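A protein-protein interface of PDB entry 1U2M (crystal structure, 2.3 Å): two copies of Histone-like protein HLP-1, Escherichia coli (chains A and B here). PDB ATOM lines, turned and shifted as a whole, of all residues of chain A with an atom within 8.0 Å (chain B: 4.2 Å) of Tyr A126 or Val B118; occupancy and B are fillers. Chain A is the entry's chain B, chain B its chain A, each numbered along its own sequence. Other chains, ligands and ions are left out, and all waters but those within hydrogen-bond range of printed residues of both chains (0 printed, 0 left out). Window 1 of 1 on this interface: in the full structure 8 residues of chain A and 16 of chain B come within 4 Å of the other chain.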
ATOM      1  N   ILE A   8      20.287 -11.161 -18.071  1.00  0.00           N
ATOM      2  CA  ILE A   8      20.081 -11.158 -19.508  1.00  0.00           C
ATOM      3  C   ILE A   8      20.633  -9.842 -20.042  1.00  0.00           C
ATOM      4  O   ILE A   8      20.768  -8.854 -19.295  1.00  0.00           O
ATOM      5  CB  ILE A   8      18.581 -11.314 -19.920  1.00  0.00           C
ATOM      6  CG1 ILE A   8      17.728 -10.157 -19.406  1.00  0.00           C
ATOM      7  CG2 ILE A   8      18.041 -12.660 -19.394  1.00  0.00           C
ATOM      8  CD1 ILE A   8      16.264 -10.193 -19.967  1.00  0.00           C
ATOM      9  N   VAL A 119      22.744 -14.379 -20.291  1.00  0.00           N
ATOM     10  CA  VAL A 119      22.146 -14.934 -21.511  1.00  0.00           C
ATOM     11  C   VAL A 119      21.634 -13.818 -22.433  1.00  0.00           C
ATOM     12  O   VAL A 119      21.103 -12.802 -21.966  1.00  0.00           O
ATOM     13  CB  VAL A 119      20.927 -15.841 -21.145  1.00  0.00           C
ATOM     14  CG1 VAL A 119      20.415 -16.559 -22.387  1.00  0.00           C
ATOM     15  CG2 VAL A 119      21.313 -16.824 -20.049  1.00  0.00           C
ATOM     16  N   ASP A 120      21.782 -14.022 -23.734  1.00  0.00           N
ATOM     17  CA  ASP A 120      21.328 -13.071 -24.750  1.00  0.00           C
ATOM     18  C   ASP A 120      19.780 -13.008 -24.648  1.00  0.00           C
ATOM     19  O   ASP A 120      19.094 -14.038 -24.735  1.00  0.00           O
ATOM     20  CB  ASP A 120      21.757 -13.594 -26.135  1.00  0.00           C
ATOM     21  CG  ASP A 120      21.521 -12.583 -27.274  1.00  0.00           C
ATOM     22  OD1 ASP A 120      20.651 -11.687 -27.165  1.00  0.00           O
ATOM     23  OD2 ASP A 120      22.212 -12.707 -28.302  1.00  0.00           O
ATOM     24  N   ALA A 121      19.232 -11.812 -24.454  1.00  0.00           N
ATOM     25  CA  ALA A 121      17.774 -11.666 -24.320  1.00  0.00           C
ATOM     26  C   ALA A 121      17.005 -12.262 -25.498  1.00  0.00           C
ATOM     27  O   ALA A 121      15.866 -12.690 -25.350  1.00  0.00           O
ATOM     28  CB  ALA A 121      17.381 -10.164 -24.142  1.00  0.00           C
ATOM     29  N   ALA A 123      17.203 -15.019 -26.660  1.00  0.00           N
ATOM     30  CA  ALA A 123      16.998 -16.452 -26.440  1.00  0.00           C
ATOM     31  C   ALA A 123      16.129 -16.653 -25.206  1.00  0.00           C
ATOM     32  O   ALA A 123      15.959 -17.781 -24.729  1.00  0.00           O
ATOM     33  CB  ALA A 123      18.368 -17.165 -26.239  1.00  0.00           C
ATOM     34  N   VAL A 124      15.575 -15.558 -24.693  1.00  0.00           N
ATOM     35  CA  VAL A 124      14.759 -15.615 -23.479  1.00  0.00           C
ATOM     36  C   VAL A 124      13.293 -15.219 -23.730  1.00  0.00           C
ATOM     37  O   VAL A 124      13.024 -14.157 -24.270  1.00  0.00           O
ATOM     38  CB  VAL A 124      15.387 -14.689 -22.419  1.00  0.00           C
ATOM     39  CG1 VAL A 124      14.478 -14.550 -21.205  1.00  0.00           C
ATOM     40  CG2 VAL A 124      16.754 -15.259 -22.023  1.00  0.00           C
ATOM     41  N   ALA A 125      12.352 -16.069 -23.333  1.00  0.00           N
ATOM     42  CA  ALA A 125      10.925 -15.772 -23.549  1.00  0.00           C
ATOM     43  C   ALA A 125      10.277 -15.145 -22.319  1.00  0.00           C
ATOM     44  O   ALA A 125       9.213 -14.537 -22.409  1.00  0.00           O
ATOM     45  CB  ALA A 125      10.157 -17.069 -23.982  1.00  0.00           C
ATOM     46  N   TYR A 126      10.919 -15.286 -21.166  1.00  0.00           N
ATOM     47  CA  TYR A 126      10.410 -14.684 -19.928  1.00  0.00           C
ATOM     48  C   TYR A 126      11.480 -14.689 -18.852  1.00  0.00           C
ATOM     49  O   TYR A 126      12.243 -15.647 -18.733  1.00  0.00           O
ATOM     50  CB  TYR A 126       9.214 -15.458 -19.342  1.00  0.00           C
ATOM     51  CG  TYR A 126       8.659 -14.794 -18.084  1.00  0.00           C
ATOM     52  CD1 TYR A 126       7.989 -13.567 -18.156  1.00  0.00           C
ATOM     53  CD2 TYR A 126       8.880 -15.334 -16.834  1.00  0.00           C
ATOM     54  CE1 TYR A 126       7.554 -12.891 -16.998  1.00  0.00           C
ATOM     55  CE2 TYR A 126       8.461 -14.673 -15.672  1.00  0.00           C
ATOM     56  CZ  TYR A 126       7.794 -13.450 -15.763  1.00  0.00           C
ATOM     57  OH  TYR A 126       7.348 -12.810 -14.624  1.00  0.00           O
ATOM     58  N   ASN A 127      11.518 -13.628 -18.058  1.00  0.00           N
ATOM     59  CA  ASN A 127      12.445 -13.564 -16.940  1.00  0.00           C
ATOM     60  C   ASN A 127      11.792 -12.785 -15.804  1.00  0.00           C
ATOM     61  O   ASN A 127      11.150 -11.757 -16.026  1.00  0.00           O
ATOM     62  CB  ASN A 127      13.807 -12.953 -17.352  1.00  0.00           C
ATOM     63  CG  ASN A 127      13.726 -11.465 -17.714  1.00  0.00           C
ATOM     64  OD1 ASN A 127      14.214 -10.611 -16.978  1.00  0.00           O
ATOM     65  ND2 ASN A 127      13.115 -11.160 -18.844  1.00  0.00           N
ATOM     66  N   SER A 128      11.914 -13.306 -14.583  1.00  0.00           N
ATOM     67  CA  SER A 128      11.345 -12.635 -13.421  1.00  0.00           C
ATOM     68  C   SER A 128      12.289 -11.469 -13.041  1.00  0.00           C
ATOM     69  O   SER A 128      13.384 -11.356 -13.610  1.00  0.00           O
ATOM     70  CB  SER A 128      11.281 -13.609 -12.266  1.00  0.00           C
ATOM     71  OG  SER A 128      12.603 -13.896 -11.880  1.00  0.00           O
ATOM     72  N   SER A 129      11.895 -10.638 -12.066  1.00  0.00           N
ATOM     73  CA  SER A 129      12.745  -9.497 -11.650  1.00  0.00           C
ATOM     74  C   SER A 129      14.075  -9.936 -11.043  1.00  0.00           C
ATOM     75  O   SER A 129      15.048  -9.175 -11.069  1.00  0.00           O
ATOM     76  CB  SER A 129      12.021  -8.544 -10.665  1.00  0.00           C
ATOM     77  OG  SER A 129      11.696  -9.189  -9.446  1.00  0.00           O
ATOM     78  N   VAL A 131      15.993 -11.870 -12.327  1.00  0.00           N
ATOM     79  CA  VAL A 131      16.913 -12.086 -13.445  1.00  0.00           C
ATOM     80  C   VAL A 131      17.051 -10.720 -14.087  1.00  0.00           C
ATOM     81  O   VAL A 131      16.246 -10.307 -14.928  1.00  0.00           O
ATOM     82  CB  VAL A 131      16.354 -13.128 -14.416  1.00  0.00           C
ATOM     83  CG1 VAL A 131      17.218 -13.202 -15.685  1.00  0.00           C
ATOM     84  CG2 VAL A 131      16.291 -14.514 -13.688  1.00  0.00           C
ATOM     85  N   ALA B   7      13.007 -22.981 -17.294  1.00  0.00           N
ATOM     86  CA  ALA B   7      12.232 -23.859 -18.153  1.00  0.00           C
ATOM     87  C   ALA B   7      12.548 -23.521 -19.593  1.00  0.00           C
ATOM     88  O   ALA B   7      13.194 -22.510 -19.885  1.00  0.00           O
ATOM     89  CB  ALA B   7      10.709 -23.722 -17.893  1.00  0.00           C
ATOM     90  N   VAL B   9      10.926 -23.364 -23.727  1.00  0.00           N
ATOM     91  CA  VAL B   9       9.730 -23.252 -24.522  1.00  0.00           C
ATOM     92  C   VAL B   9      10.160 -23.202 -25.984  1.00  0.00           C
ATOM     93  O   VAL B   9      11.171 -22.581 -26.334  1.00  0.00           O
ATOM     94  CB  VAL B   9       8.910 -21.995 -24.152  1.00  0.00           C
ATOM     95  CG1 VAL B   9       9.641 -20.727 -24.588  1.00  0.00           C
ATOM     96  CG2 VAL B   9       7.530 -22.086 -24.800  1.00  0.00           C
ATOM     97  N   VAL B 106       3.317 -17.239 -22.291  1.00  0.00           N
ATOM     98  CA  VAL B 106       4.530 -17.743 -21.644  1.00  0.00           C
ATOM     99  C   VAL B 106       4.632 -17.168 -20.222  1.00  0.00           C
ATOM    100  O   VAL B 106       4.864 -17.890 -19.244  1.00  0.00           O
ATOM    101  CB  VAL B 106       5.784 -17.334 -22.420  1.00  0.00           C
ATOM    102  CG1 VAL B 106       7.037 -17.661 -21.588  1.00  0.00           C
ATOM    103  CG2 VAL B 106       5.815 -18.056 -23.764  1.00  0.00           C
ATOM    104  N   LYS B 107       4.424 -15.866 -20.109  1.00  0.00           N
ATOM    105  CA  LYS B 107       4.487 -15.183 -18.812  1.00  0.00           C
ATOM    106  C   LYS B 107       3.454 -15.769 -17.837  1.00  0.00           C
ATOM    107  O   LYS B 107       3.747 -16.045 -16.678  1.00  0.00           O
ATOM    108  CB  LYS B 107       4.224 -13.694 -19.032  1.00  0.00           C
ATOM    109  CG  LYS B 107       4.216 -12.838 -17.760  1.00  0.00           C
ATOM    110  CD  LYS B 107       4.098 -11.360 -18.158  1.00  0.00           C
ATOM    111  CE  LYS B 107       4.054 -10.451 -16.957  1.00  0.00           C
ATOM    112  NZ  LYS B 107       3.759  -9.057 -17.402  1.00  0.00           N
ATOM    113  N   ALA B 110       4.651 -19.193 -16.788  1.00  0.00           N
ATOM    114  CA  ALA B 110       5.842 -19.082 -15.951  1.00  0.00           C
ATOM    115  C   ALA B 110       5.452 -18.728 -14.518  1.00  0.00           C
ATOM    116  O   ALA B 110       5.954 -19.339 -13.558  1.00  0.00           O
ATOM    117  CB  ALA B 110       6.813 -18.014 -16.523  1.00  0.00           C
ATOM    118  N   ASN B 111       4.556 -17.749 -14.361  1.00  0.00           N
ATOM    119  CA  ASN B 111       4.143 -17.356 -13.013  1.00  0.00           C
ATOM    120  C   ASN B 111       3.391 -18.479 -12.345  1.00  0.00           C
ATOM    121  O   ASN B 111       3.626 -18.795 -11.180  1.00  0.00           O
ATOM    122  CB  ASN B 111       3.296 -16.088 -13.063  1.00  0.00           C
ATOM    123  CG  ASN B 111       4.158 -14.874 -13.214  1.00  0.00           C
ATOM    124  OD1 ASN B 111       4.448 -14.415 -14.335  1.00  0.00           O
ATOM    125  ND2 ASN B 111       4.639 -14.372 -12.083  1.00  0.00           N
ATOM    126  N   ILE B 115       8.329 -20.152 -12.443  1.00  0.00           N
ATOM    127  CA  ILE B 115       9.558 -20.238 -13.206  1.00  0.00           C
ATOM    128  C   ILE B 115      10.138 -18.826 -13.330  1.00  0.00           C
ATOM    129  O   ILE B 115       9.421 -17.903 -13.690  1.00  0.00           O
ATOM    130  CB  ILE B 115       9.250 -20.822 -14.605  1.00  0.00           C
ATOM    131  CG1 ILE B 115       8.764 -22.267 -14.437  1.00  0.00           C
ATOM    132  CG2 ILE B 115      10.490 -20.729 -15.524  1.00  0.00           C
ATOM    133  CD1 ILE B 115       7.932 -22.769 -15.623  1.00  0.00           C
ATOM    134  N   ASP B 116      11.427 -18.664 -13.036  1.00  0.00           N
ATOM    135  CA  ASP B 116      12.106 -17.359 -13.134  1.00  0.00           C
ATOM    136  C   ASP B 116      12.677 -17.056 -14.493  1.00  0.00           C
ATOM    137  O   ASP B 116      12.872 -15.890 -14.860  1.00  0.00           O
ATOM    138  CB  ASP B 116      13.278 -17.263 -12.160  1.00  0.00           C
ATOM    139  CG  ASP B 116      12.833 -17.136 -10.738  1.00  0.00           C
ATOM    140  OD1 ASP B 116      12.149 -16.133 -10.431  1.00  0.00           O
ATOM    141  OD2 ASP B 116      13.165 -18.038  -9.936  1.00  0.00           O
ATOM    142  N   LEU B 117      12.992 -18.103 -15.239  1.00  0.00           N
ATOM    143  CA  LEU B 117      13.595 -17.880 -16.543  1.00  0.00           C
ATOM    144  C   LEU B 117      13.160 -18.939 -17.516  1.00  0.00           C
ATOM    145  O   LEU B 117      13.313 -20.140 -17.251  1.00  0.00           O
ATOM    146  CB  LEU B 117      15.130 -17.902 -16.423  1.00  0.00           C
ATOM    147  CG  LEU B 117      15.859 -17.822 -17.770  1.00  0.00           C
ATOM    148  CD1 LEU B 117      15.812 -16.392 -18.242  1.00  0.00           C
ATOM    149  CD2 LEU B 117      17.338 -18.281 -17.639  1.00  0.00           C
ATOM    150  N   VAL B 118      12.607 -18.498 -18.632  1.00  0.00           N
ATOM    151  CA  VAL B 118      12.194 -19.412 -19.673  1.00  0.00           C
ATOM    152  C   VAL B 118      13.075 -19.144 -20.897  1.00  0.00           C
ATOM    153  O   VAL B 118      13.070 -18.037 -21.443  1.00  0.00           O
ATOM    154  CB  VAL B 118      10.728 -19.195 -20.091  1.00  0.00           C
ATOM    155  CG1 VAL B 118      10.357 -20.219 -21.167  1.00  0.00           C
ATOM    156  CG2 VAL B 118       9.818 -19.317 -18.888  1.00  0.00           C
ATOM    157  N   VAL B 119      13.796 -20.178 -21.327  1.00  0.00           N
ATOM    158  CA  VAL B 119      14.704 -20.123 -22.467  1.00  0.00           C
ATOM    159  C   VAL B 119      14.101 -20.741 -23.747  1.00  0.00           C
ATOM    160  O   VAL B 119      13.388 -21.753 -23.689  1.00  0.00           O
ATOM    161  CB  VAL B 119      16.016 -20.896 -22.131  1.00  0.00           C
ATOM    162  CG1 VAL B 119      17.003 -20.758 -23.270  1.00  0.00           C
ATOM    163  CG2 VAL B 119      16.632 -20.350 -20.861  1.00  0.00           C
ATOM    164  N   ILE B 134       7.652 -26.162 -21.267  1.00  0.00           N
ATOM    165  CA  ILE B 134       6.280 -25.701 -21.037  1.00  0.00           C
ATOM    166  C   ILE B 134       5.543 -25.359 -22.317  1.00  0.00           C
ATOM    167  O   ILE B 134       4.510 -24.678 -22.283  1.00  0.00           O
ATOM    168  CB  ILE B 134       6.260 -24.448 -20.123  1.00  0.00           C
ATOM    169  CG1 ILE B 134       7.093 -23.323 -20.757  1.00  0.00           C
ATOM    170  CG2 ILE B 134       6.796 -24.805 -18.766  1.00  0.00           C
ATOM    171  CD1 ILE B 134       6.866 -21.966 -20.154  1.00  0.00           C
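Tyr A126 touches just these residues of chain B: Val B106 (3.8 Å), Lys B107 (3.4 Å), Ala B110 (3.4 Å), Asn B111 (3.3 Å), Ile B115 (3.9 Å), Asp B116 (3.9 Å), Leu B117 (3.4 Å) and Val B118 (2.9 Å).
Val B118 touches just these residues of chain A: Val A124, Ala A125 and Tyr A126.
Printed residues of chain A within 4 Å of Leu B117: Val A124 and Tyr A126.
Of the printed residues of chain B, Ser A128 touches Asp B116 (2.7 Å).
Ile B134 touches none of the printed residues of chain A.
Ser A129 touches none of the printed residues of chain B.
The nearest residue of chain A that does not touch Val B118 is Ala A123 (4.4 Å).
Printed residues of chain B that touch a printed residue of chain A: Val B9, Val B106, Lys B107, Ala B110, Asn B111, Ile B115, Asp B116, Leu B117, Val B118 and Val B119.
Among the printed residues, 17 pairs touch across the chains.
Among the printed residues, pairs that only touch across the chains: Asn A127 with Asp B116, Tyr A126 with Ala B110, Tyr A126 with Leu B117, Tyr A126 with Lys B107, Ala A123 with Val B119, Val A124 with Val B118, Val A124 with Leu B117, Ala A125 with Val B9, Tyr A126 with Val B106, Val A131 with Asp B116, Ala A125 with Val B106, Tyr A126 with Ile B115 and Tyr A126 with Asp B116.
The backbone NH of Ala B7 is in hydrogen-bond range of the backbone carbonyl oxygen of Leu B117 (2.9 Å).
The backbone carbonyl oxygen (O) of Ala B7 sits at hydrogen-bond distance from the backbone NH (N) of Val B119, at 2.8 Å.
The backbone carbonyl oxygen of Val B119 is in hydrogen-bond range of the backbone NH of Val B9 (2.9 Å).
The side-chain amide oxygen of Asn B111 sits close to the backbone carbonyl oxygen of Lys B107 (2.9 Å).
The backbone NH (N) of Ile B115 is in hydrogen-bond range of the backbone carbonyl oxygen (O) of Ala B110 (2.7 Å).
The backbone carbonyl oxygen of Val A131 lies close to the side-chain amide oxygen of Asn A127 (2.9 Å).
1 position is printed for both chains.
OD1 of Asn B111 sits at hydrogen-bond distance from OH of Tyr A126, at 3.3 Å.
The side-chain carboxylate (OD1) of Asp B116 lies within hydrogen-bond range of the side-chain hydroxyl (OG) of Ser A128 (2.7 Å).
The backbone NH (N) of Ala A125 sits at hydrogen-bond distance from the backbone carbonyl oxygen (O) of Val B118, at 2.8 Å.
The backbone carbonyl oxygen (O) of Tyr A126 sits at hydrogen-bond distance from the backbone NH (N) of Val B118, at 2.9 Å.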
